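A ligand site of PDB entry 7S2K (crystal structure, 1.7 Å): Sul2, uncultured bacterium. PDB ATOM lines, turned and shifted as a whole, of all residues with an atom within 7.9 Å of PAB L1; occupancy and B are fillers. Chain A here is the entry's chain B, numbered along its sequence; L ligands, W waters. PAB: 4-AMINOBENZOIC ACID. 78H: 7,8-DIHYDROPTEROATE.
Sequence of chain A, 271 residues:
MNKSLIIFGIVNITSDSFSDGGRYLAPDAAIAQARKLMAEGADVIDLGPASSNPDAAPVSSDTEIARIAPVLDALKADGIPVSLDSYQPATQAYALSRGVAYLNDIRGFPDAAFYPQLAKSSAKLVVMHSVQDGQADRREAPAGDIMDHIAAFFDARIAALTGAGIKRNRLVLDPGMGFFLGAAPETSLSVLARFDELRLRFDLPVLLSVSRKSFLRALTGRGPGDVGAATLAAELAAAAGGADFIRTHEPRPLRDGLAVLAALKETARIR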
ATOM      1  N   ILE A  10      13.715   4.064   4.727  1.00  0.00           N
ATOM      2  CA  ILE A  10      13.871   5.325   4.007  1.00  0.00           C
ATOM      3  C   ILE A  10      14.231   5.034   2.549  1.00  0.00           C
ATOM      4  O   ILE A  10      15.238   4.367   2.267  1.00  0.00           O
ATOM      5  CB  ILE A  10      14.951   6.202   4.657  1.00  0.00           C
ATOM      6  CG1 ILE A  10      14.518   6.643   6.053  1.00  0.00           C
ATOM      7  CG2 ILE A  10      15.237   7.431   3.783  1.00  0.00           C
ATOM      8  CD1 ILE A  10      15.646   7.267   6.850  1.00  0.00           C
ATOM      9  N   VAL A  11      13.435   5.550   1.624  1.00  0.00           N
ATOM     10  CA  VAL A  11      13.772   5.563   0.202  1.00  0.00           C
ATOM     11  C   VAL A  11      13.697   7.025  -0.236  1.00  0.00           C
ATOM     12  O   VAL A  11      12.601   7.582  -0.378  1.00  0.00           O
ATOM     13  CB  VAL A  11      12.826   4.700  -0.637  1.00  0.00           C
ATOM     14  CG1 VAL A  11      13.148   4.832  -2.122  1.00  0.00           C
ATOM     15  CG2 VAL A  11      12.913   3.249  -0.205  1.00  0.00           C
ATOM     16  N   ASN A  12      14.854   7.656  -0.425  1.00  0.00           N
ATOM     17  CA  ASN A  12      14.915   9.031  -0.930  1.00  0.00           C
ATOM     18  C   ASN A  12      15.259   8.981  -2.414  1.00  0.00           C
ATOM     19  O   ASN A  12      16.284   8.393  -2.795  1.00  0.00           O
ATOM     20  CB  ASN A  12      15.944   9.858  -0.157  1.00  0.00           C
ATOM     21  CG  ASN A  12      15.453  10.274   1.231  1.00  0.00           C
ATOM     22  OD1 ASN A  12      14.342  10.780   1.384  1.00  0.00           O
ATOM     23  ND2 ASN A  12      16.302  10.086   2.233  1.00  0.00           N
ATOM     24  N   THR A  14      16.401  11.212  -4.203  1.00  0.00           N
ATOM     25  CA  THR A  14      17.658  11.912  -4.421  1.00  0.00           C
ATOM     26  C   THR A  14      18.742  11.376  -3.492  1.00  0.00           C
ATOM     27  O   THR A  14      19.887  11.181  -3.911  1.00  0.00           O
ATOM     28  CB  THR A  14      17.495  13.425  -4.209  1.00  0.00           C
ATOM     29  OG1 THR A  14      17.645  13.721  -2.818  1.00  0.00           O
ATOM     30  CG2 THR A  14      16.123  13.883  -4.674  1.00  0.00           C
ATOM     31  N   ASP A  46       9.090   4.739   3.757  1.00  0.00           N
ATOM     32  CA  ASP A  46       8.989   6.197   3.823  1.00  0.00           C
ATOM     33  C   ASP A  46       9.650   6.772   2.583  1.00  0.00           C
ATOM     34  O   ASP A  46      10.877   6.853   2.481  1.00  0.00           O
ATOM     35  CB  ASP A  46       9.636   6.743   5.089  1.00  0.00           C
ATOM     36  CG  ASP A  46       9.385   8.224   5.287  1.00  0.00           C
ATOM     37  OD1 ASP A  46       8.199   8.595   5.418  1.00  0.00           O
ATOM     38  OD2 ASP A  46      10.355   9.011   5.304  1.00  0.00           O
ATOM     39  N   GLY A  48      10.650   9.606   0.074  1.00  0.00           N
ATOM     40  CA  GLY A  48      10.889  11.029   0.059  1.00  0.00           C
ATOM     41  C   GLY A  48      11.374  11.502  -1.297  1.00  0.00           C
ATOM     42  O   GLY A  48      12.459  11.130  -1.762  1.00  0.00           O
ATOM     43  N   ALA A  50      12.274  14.580  -2.231  1.00  0.00           N
ATOM     44  CA  ALA A  50      13.184  15.720  -2.203  1.00  0.00           C
ATOM     45  C   ALA A  50      14.244  15.541  -1.115  1.00  0.00           C
ATOM     46  O   ALA A  50      14.308  14.462  -0.513  1.00  0.00           O
ATOM     47  CB  ALA A  50      12.403  17.020  -1.971  1.00  0.00           C
ATOM     48  N   SER A  51      15.063  16.545  -0.818  1.00  0.00           N
ATOM     49  CA  SER A  51      15.853  16.449   0.410  1.00  0.00           C
ATOM     50  C   SER A  51      15.801  17.674   1.280  1.00  0.00           C
ATOM     51  O   SER A  51      16.235  18.779   0.901  1.00  0.00           O
ATOM     52  CB  SER A  51      17.289  16.080   0.168  1.00  0.00           C
ATOM     53  OG  SER A  51      18.007  15.922   1.370  1.00  0.00           O
ATOM     54  N   SER A  52      15.365  17.412   2.489  1.00  0.00           N
ATOM     55  CA  SER A  52      15.326  18.185   3.707  1.00  0.00           C
ATOM     56  C   SER A  52      16.542  17.950   4.587  1.00  0.00           C
ATOM     57  O   SER A  52      16.391  17.782   5.803  1.00  0.00           O
ATOM     58  CB  SER A  52      14.054  17.762   4.417  1.00  0.00           C
ATOM     59  OG  SER A  52      14.065  16.337   4.516  1.00  0.00           O
ATOM     60  N   ASN A  53      17.743  17.887   4.031  1.00  0.00           N
ATOM     61  CA  ASN A  53      18.972  17.895   4.810  1.00  0.00           C
ATOM     62  C   ASN A  53      19.198  19.316   5.295  1.00  0.00           C
ATOM     63  O   ASN A  53      18.359  20.192   5.060  1.00  0.00           O
ATOM     64  CB  ASN A  53      20.120  17.368   3.953  1.00  0.00           C
ATOM     65  CG  ASN A  53      19.858  15.988   3.445  1.00  0.00           C
ATOM     66  OD1 ASN A  53      20.396  15.588   2.417  1.00  0.00           O
ATOM     67  ND2 ASN A  53      19.017  15.253   4.156  1.00  0.00           N
ATOM     68  N   PRO A  54      20.306  19.612   5.976  1.00  0.00           N
ATOM     69  CA  PRO A  54      20.641  21.035   6.131  1.00  0.00           C
ATOM     70  C   PRO A  54      20.965  21.676   4.798  1.00  0.00           C
ATOM     71  O   PRO A  54      20.714  22.868   4.623  1.00  0.00           O
ATOM     72  CB  PRO A  54      21.848  21.040   7.082  1.00  0.00           C
ATOM     73  CG  PRO A  54      22.398  19.681   7.024  1.00  0.00           C
ATOM     74  CD  PRO A  54      21.239  18.765   6.758  1.00  0.00           C
ATOM     75  N   ASP A  85       7.000  11.204   2.536  1.00  0.00           N
ATOM     76  CA  ASP A  85       7.780  12.205   3.249  1.00  0.00           C
ATOM     77  C   ASP A  85       7.866  13.451   2.364  1.00  0.00           C
ATOM     78  O   ASP A  85       8.768  13.595   1.542  1.00  0.00           O
ATOM     79  CB  ASP A  85       9.162  11.655   3.599  1.00  0.00           C
ATOM     80  CG  ASP A  85      10.051  12.668   4.304  1.00  0.00           C
ATOM     81  OD1 ASP A  85       9.581  13.775   4.644  1.00  0.00           O
ATOM     82  OD2 ASP A  85      11.223  12.333   4.544  1.00  0.00           O
ATOM     83  N   PHE A 180      17.152  19.458  13.030  1.00  0.00           N
ATOM     84  CA  PHE A 180      15.803  19.921  13.339  1.00  0.00           C
ATOM     85  C   PHE A 180      15.681  20.404  14.770  1.00  0.00           C
ATOM     86  O   PHE A 180      14.672  21.051  15.110  1.00  0.00           O
ATOM     87  CB  PHE A 180      14.778  18.809  13.093  1.00  0.00           C
ATOM     88  CG  PHE A 180      14.587  18.461  11.636  1.00  0.00           C
ATOM     89  CD1 PHE A 180      14.320  19.445  10.705  1.00  0.00           C
ATOM     90  CD2 PHE A 180      14.636  17.134  11.220  1.00  0.00           C
ATOM     91  CE1 PHE A 180      14.123  19.129   9.369  1.00  0.00           C
ATOM     92  CE2 PHE A 180      14.428  16.807   9.890  1.00  0.00           C
ATOM     93  CZ  PHE A 180      14.178  17.814   8.956  1.00  0.00           C
ATOM     94  N   SER A 209      13.715   9.376  14.176  1.00  0.00           N
ATOM     95  CA  SER A 209      14.579   9.169  13.022  1.00  0.00           C
ATOM     96  C   SER A 209      15.963   9.704  13.383  1.00  0.00           C
ATOM     97  O   SER A 209      16.239  10.893  13.243  1.00  0.00           O
ATOM     98  CB  SER A 209      14.027   9.844  11.776  1.00  0.00           C
ATOM     99  OG  SER A 209      14.696   9.365  10.621  1.00  0.00           O
ATOM    100  N   VAL A 210      16.839   8.819  13.858  1.00  0.00           N
ATOM    101  CA  VAL A 210      18.215   9.194  14.156  1.00  0.00           C
ATOM    102  C   VAL A 210      19.172   8.794  13.032  1.00  0.00           C
ATOM    103  O   VAL A 210      20.304   9.314  12.997  1.00  0.00           O
ATOM    104  CB  VAL A 210      18.694   8.571  15.483  1.00  0.00           C
ATOM    105  CG1 VAL A 210      17.811   9.023  16.634  1.00  0.00           C
ATOM    106  CG2 VAL A 210      18.700   7.052  15.367  1.00  0.00           C
ATOM    107  N   SER A 211      18.761   7.902  12.142  1.00  0.00           N
ATOM    108  CA  SER A 211      19.650   7.276  11.168  1.00  0.00           C
ATOM    109  C   SER A 211      20.508   8.288  10.415  1.00  0.00           C
ATOM    110  O   SER A 211      19.988   9.182   9.738  1.00  0.00           O
ATOM    111  CB  SER A 211      18.819   6.452  10.184  1.00  0.00           C
ATOM    112  OG  SER A 211      19.639   5.617   9.392  1.00  0.00           O
ATOM    113  N   ARG A 212      21.832   8.130  10.533  1.00  0.00           N
ATOM    114  CA  ARG A 212      22.865   8.887   9.827  1.00  0.00           C
ATOM    115  C   ARG A 212      22.824  10.383  10.086  1.00  0.00           C
ATOM    116  O   ARG A 212      23.395  11.164   9.323  1.00  0.00           O
ATOM    117  CB  ARG A 212      22.817   8.622   8.319  1.00  0.00           C
ATOM    118  CG  ARG A 212      23.018   7.163   7.964  1.00  0.00           C
ATOM    119  CD  ARG A 212      22.697   6.881   6.509  1.00  0.00           C
ATOM    120  NE  ARG A 212      22.802   5.450   6.247  1.00  0.00           N
ATOM    121  CZ  ARG A 212      22.651   4.890   5.057  1.00  0.00           C
ATOM    122  NH1 ARG A 212      22.383   5.607   3.981  1.00  0.00           N
ATOM    123  NH2 ARG A 212      22.754   3.571   4.948  1.00  0.00           N
ATOM    124  N   LYS A 213      22.196  10.835  11.163  1.00  0.00           N
ATOM    125  CA  LYS A 213      22.146  12.266  11.410  1.00  0.00           C
ATOM    126  C   LYS A 213      23.485  12.755  11.967  1.00  0.00           C
ATOM    127  O   LYS A 213      24.249  11.986  12.579  1.00  0.00           O
ATOM    128  CB  LYS A 213      21.000  12.610  12.348  1.00  0.00           C
ATOM    129  CG  LYS A 213      19.628  12.363  11.733  1.00  0.00           C
ATOM    130  CD  LYS A 213      18.619  13.381  12.222  1.00  0.00           C
ATOM    131  CE  LYS A 213      17.505  13.625  11.215  1.00  0.00           C
ATOM    132  NZ  LYS A 213      16.664  12.433  10.941  1.00  0.00           N
ATOM    133  N   SER A 214      23.773  14.040  11.770  1.00  0.00           N
ATOM    134  CA  SER A 214      25.128  14.513  12.003  1.00  0.00           C
ATOM    135  C   SER A 214      25.534  14.472  13.470  1.00  0.00           C
ATOM    136  O   SER A 214      26.736  14.390  13.745  1.00  0.00           O
ATOM    137  CB  SER A 214      25.312  15.939  11.461  1.00  0.00           C
ATOM    138  OG  SER A 214      24.134  16.703  11.629  1.00  0.00           O
ATOM    139  N   ARG A 217      27.736  11.688  14.214  1.00  0.00           N
ATOM    140  CA  ARG A 217      29.115  11.869  13.754  1.00  0.00           C
ATOM    141  C   ARG A 217      29.964  12.564  14.802  1.00  0.00           C
ATOM    142  O   ARG A 217      31.152  12.254  14.934  1.00  0.00           O
ATOM    143  CB  ARG A 217      29.120  12.662  12.437  1.00  0.00           C
ATOM    144  CG  ARG A 217      28.388  11.943  11.341  1.00  0.00           C
ATOM    145  CD  ARG A 217      28.512  12.619   9.985  1.00  0.00           C
ATOM    146  NE  ARG A 217      27.473  12.122   9.103  1.00  0.00           N
ATOM    147  CZ  ARG A 217      27.565  10.982   8.412  1.00  0.00           C
ATOM    148  NH1 ARG A 217      28.649  10.221   8.479  1.00  0.00           N
ATOM    149  NH2 ARG A 217      26.547  10.604   7.638  1.00  0.00           N
ATOM    150  N   VAL A 227      28.609   5.726   9.799  1.00  0.00           N
ATOM    151  CA  VAL A 227      27.970   5.887  11.107  1.00  0.00           C
ATOM    152  C   VAL A 227      26.847   4.868  11.353  1.00  0.00           C
ATOM    153  O   VAL A 227      25.891   5.143  12.093  1.00  0.00           O
ATOM    154  CB  VAL A 227      27.393   7.308  11.308  1.00  0.00           C
ATOM    155  CG1 VAL A 227      28.498   8.340  11.259  1.00  0.00           C
ATOM    156  CG2 VAL A 227      26.298   7.614  10.273  1.00  0.00           C
ATOM    157  N   ARG A 247      12.339   5.305  11.999  1.00  0.00           N
ATOM    158  CA  ARG A 247      12.540   5.559  10.576  1.00  0.00           C
ATOM    159  C   ARG A 247      14.034   5.449  10.315  1.00  0.00           C
ATOM    160  O   ARG A 247      14.823   6.174  10.936  1.00  0.00           O
ATOM    161  CB  ARG A 247      12.005   6.943  10.204  1.00  0.00           C
ATOM    162  CG  ARG A 247      12.477   7.491   8.870  1.00  0.00           C
ATOM    163  CD  ARG A 247      11.824   8.835   8.583  1.00  0.00           C
ATOM    164  NE  ARG A 247      12.187   9.363   7.268  1.00  0.00           N
ATOM    165  CZ  ARG A 247      13.364   9.895   6.970  1.00  0.00           C
ATOM    166  NH1 ARG A 247      14.306  10.063   7.876  1.00  0.00           N
ATOM    167  NH2 ARG A 247      13.593  10.291   5.715  1.00  0.00           N
ATOM    168  N   THR A 248      14.429   4.536   9.436  1.00  0.00           N
ATOM    169  CA  THR A 248      15.844   4.207   9.318  1.00  0.00           C
ATOM    170  C   THR A 248      16.213   3.890   7.878  1.00  0.00           C
ATOM    171  O   THR A 248      15.372   3.502   7.067  1.00  0.00           O
ATOM    172  CB  THR A 248      16.216   3.022  10.218  1.00  0.00           C
ATOM    173  OG1 THR A 248      17.637   2.837  10.197  1.00  0.00           O
ATOM    174  CG2 THR A 248      15.539   1.753   9.731  1.00  0.00           C
ATOM    175  N   HIS A 249      17.508   4.040   7.567  1.00  0.00           N
ATOM    176  CA  HIS A 249      18.031   3.637   6.266  1.00  0.00           C
ATOM    177  C   HIS A 249      18.292   2.139   6.190  1.00  0.00           C
ATOM    178  O   HIS A 249      18.246   1.569   5.095  1.00  0.00           O
ATOM    179  CB  HIS A 249      19.327   4.379   5.953  1.00  0.00           C
ATOM    180  CG  HIS A 249      19.166   5.862   5.833  1.00  0.00           C
ATOM    181  ND1 HIS A 249      19.330   6.725   6.908  1.00  0.00           N
ATOM    182  CD2 HIS A 249      18.868   6.648   4.771  1.00  0.00           C
ATOM    183  CE1 HIS A 249      19.140   7.961   6.511  1.00  0.00           C
ATOM    184  NE2 HIS A 249      18.848   7.945   5.217  1.00  0.00           N
HETATM  185  C1' PAB L   1      17.040  11.171   6.086  1.00  0.00           C
HETATM  186  O1' PAB L   1      16.613  10.834   7.214  1.00  0.00           O
HETATM  187  O2' PAB L   1      16.288  11.172   5.082  1.00  0.00           O
HETATM  188  C1  PAB L   1      18.492  11.606   5.950  1.00  0.00           C
HETATM  189  C2  PAB L   1      19.297  11.522   7.059  1.00  0.00           C
HETATM  190  C3  PAB L   1      20.622  11.920   6.981  1.00  0.00           C
HETATM  191  C4  PAB L   1      21.106  12.401   5.773  1.00  0.00           C
HETATM  192  C5  PAB L   1      20.293  12.482   4.659  1.00  0.00           C
HETATM  193  C6  PAB L   1      18.968  12.084   4.738  1.00  0.00           C
HETATM  194  N4  PAB L   1      22.493  12.810   5.683  1.00  0.00           N
HETATM  195  O4  78H L   2      13.890  13.230  11.408  1.00  0.00           O
HETATM  196  C4  78H L   2      13.033  13.021  10.565  1.00  0.00           C
HETATM  197  C5  78H L   2      13.288  13.187   9.224  1.00  0.00           C
HETATM  198  N3  78H L   2      11.727  12.664  10.951  1.00  0.00           N
HETATM  199  C9  78H L   2      12.283  12.973   8.309  1.00  0.00           C
HETATM  200  N5  78H L   2      14.513  13.495   8.841  1.00  0.00           N
HETATM  201  C2  78H L   2      10.734  12.464   9.984  1.00  0.00           C
HETATM  202  N8  78H L   2      12.571  13.114   6.965  1.00  0.00           N
HETATM  203  N1  78H L   2      11.045  12.640   8.686  1.00  0.00           N
HETATM  204  C6  78H L   2      14.780  13.783   7.580  1.00  0.00           C
HETATM  205  N2  78H L   2       9.511  12.152  10.346  1.00  0.00           N
HETATM  206  C7  78H L   2      13.780  13.821   6.616  1.00  0.00           C
HETATM  207  C10 78H L   2      16.071  14.066   7.155  1.00  0.00           C
HETATM  208  N11 78H L   2      16.567  15.444   7.324  1.00  0.00           N
HETATM  209  C15 78H L   2      17.675  15.633   8.046  1.00  0.00           C
HETATM  210  C16 78H L   2      18.813  14.913   7.773  1.00  0.00           C
HETATM  211  C17 78H L   2      17.699  16.534   9.095  1.00  0.00           C
HETATM  212  C18 78H L   2      19.936  15.088   8.562  1.00  0.00           C
HETATM  213  C19 78H L   2      18.795  16.704   9.892  1.00  0.00           C
HETATM  214  C20 78H L   2      19.930  15.981   9.606  1.00  0.00           C
HETATM  215  C21 78H L   2      21.025  16.113  10.428  1.00  0.00           C
HETATM  216  O22 78H L   2      22.070  15.633  10.098  1.00  0.00           O
HETATM  217  O23 78H L   2      20.897  16.535  11.538  1.00  0.00           O
HETATM  218  O   HOH W   1      17.519  10.109   9.551  1.00  0.00           O
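The guanidinium group of Arg 247 lies within salt-bridge range of an oxygen (O1') of PAB L1, 2.5 Å away.
An oxygen (O2') of PAB L1 is in hydrogen-bond range of the side-chain amide nitrogen (ND2) of Asn 12, 3.0 Å away.
The guanidinium group (NH2) of Arg 247 lies close to a nitrogen (N8) of 78H L2, 3.3 Å away.
O4 of 78H L2 is in hydrogen-bond range of NZ of Lys 213.
N8 of 78H L2 sits at hydrogen-bond distance from OD2 of Asp 85 (2.9 Å).
The backbone carbonyl oxygen (O) of Ser 52 is in hydrogen-bond range of a nitrogen (N11) of 78H L2 (2.8 Å).
The backbone NH (N) of Ser 214 is in hydrogen-bond range of an oxygen (O22) of 78H L2, at 2.9 Å.
An oxygen (O22) of 78H L2 lies within hydrogen-bond range of the side-chain hydroxyl (OG) of Ser 214.
The side-chain hydroxyl of Ser 209 lies within hydrogen-bond range of the guanidinium group of Arg 247, 2.9 Å away.
The side-chain carboxylate (OD2) of Asp 85 lies within salt-bridge range of the guanidinium group (NH2) of Arg 247 (3.3 Å).
The guanidinium group of Arg 247 is in salt-bridge range of the side-chain carboxylate of Asp 46, at 2.7 Å.
OD1 of Asn 53 is in hydrogen-bond range of OG of Ser 51, 2.6 Å away.
A ring nitrogen (ND1) of His 249 is in hydrogen-bond range of the side-chain hydroxyl of Ser 211, at 2.7 Å.
The backbone NH (N) of Ile 10 lies within hydrogen-bond range of the backbone carbonyl oxygen (O) of Thr 248, at 2.9 Å.
Ile 10 touches PAB L1 (CD1 to O1', 3.7 Å).
Asn 53 touches PAB L1 (ND2 to C5, 3.1 Å).
Ser 211 touches PAB L1 (O to C2, 3.6 Å).
O of Arg 212 touches C3 of PAB L1 (3.7 Å).
His 249 touches PAB L1 (CE1 to C2, 3.6 Å).
Hydrophobic or aromatic side chains within 4 Å of PAB L1: Ile 10 and His 249.
Seven residues have an atom within 4 Å of PAB L1: Ile 10, Asn 12, Asn 53, Ser 211, Arg 212, Arg 247 and His 249.
The nearest printed residue that does not touch PAB L1 is Lys 213 (4.1 Å).
Water W1 lies within hydrogen-bond range of O1' of PAB L1 (2.6 Å), O of Ser 211 (2.6 Å), NZ of Lys 213 (2.8 Å) and OG of Ser 209 (3.1 Å).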
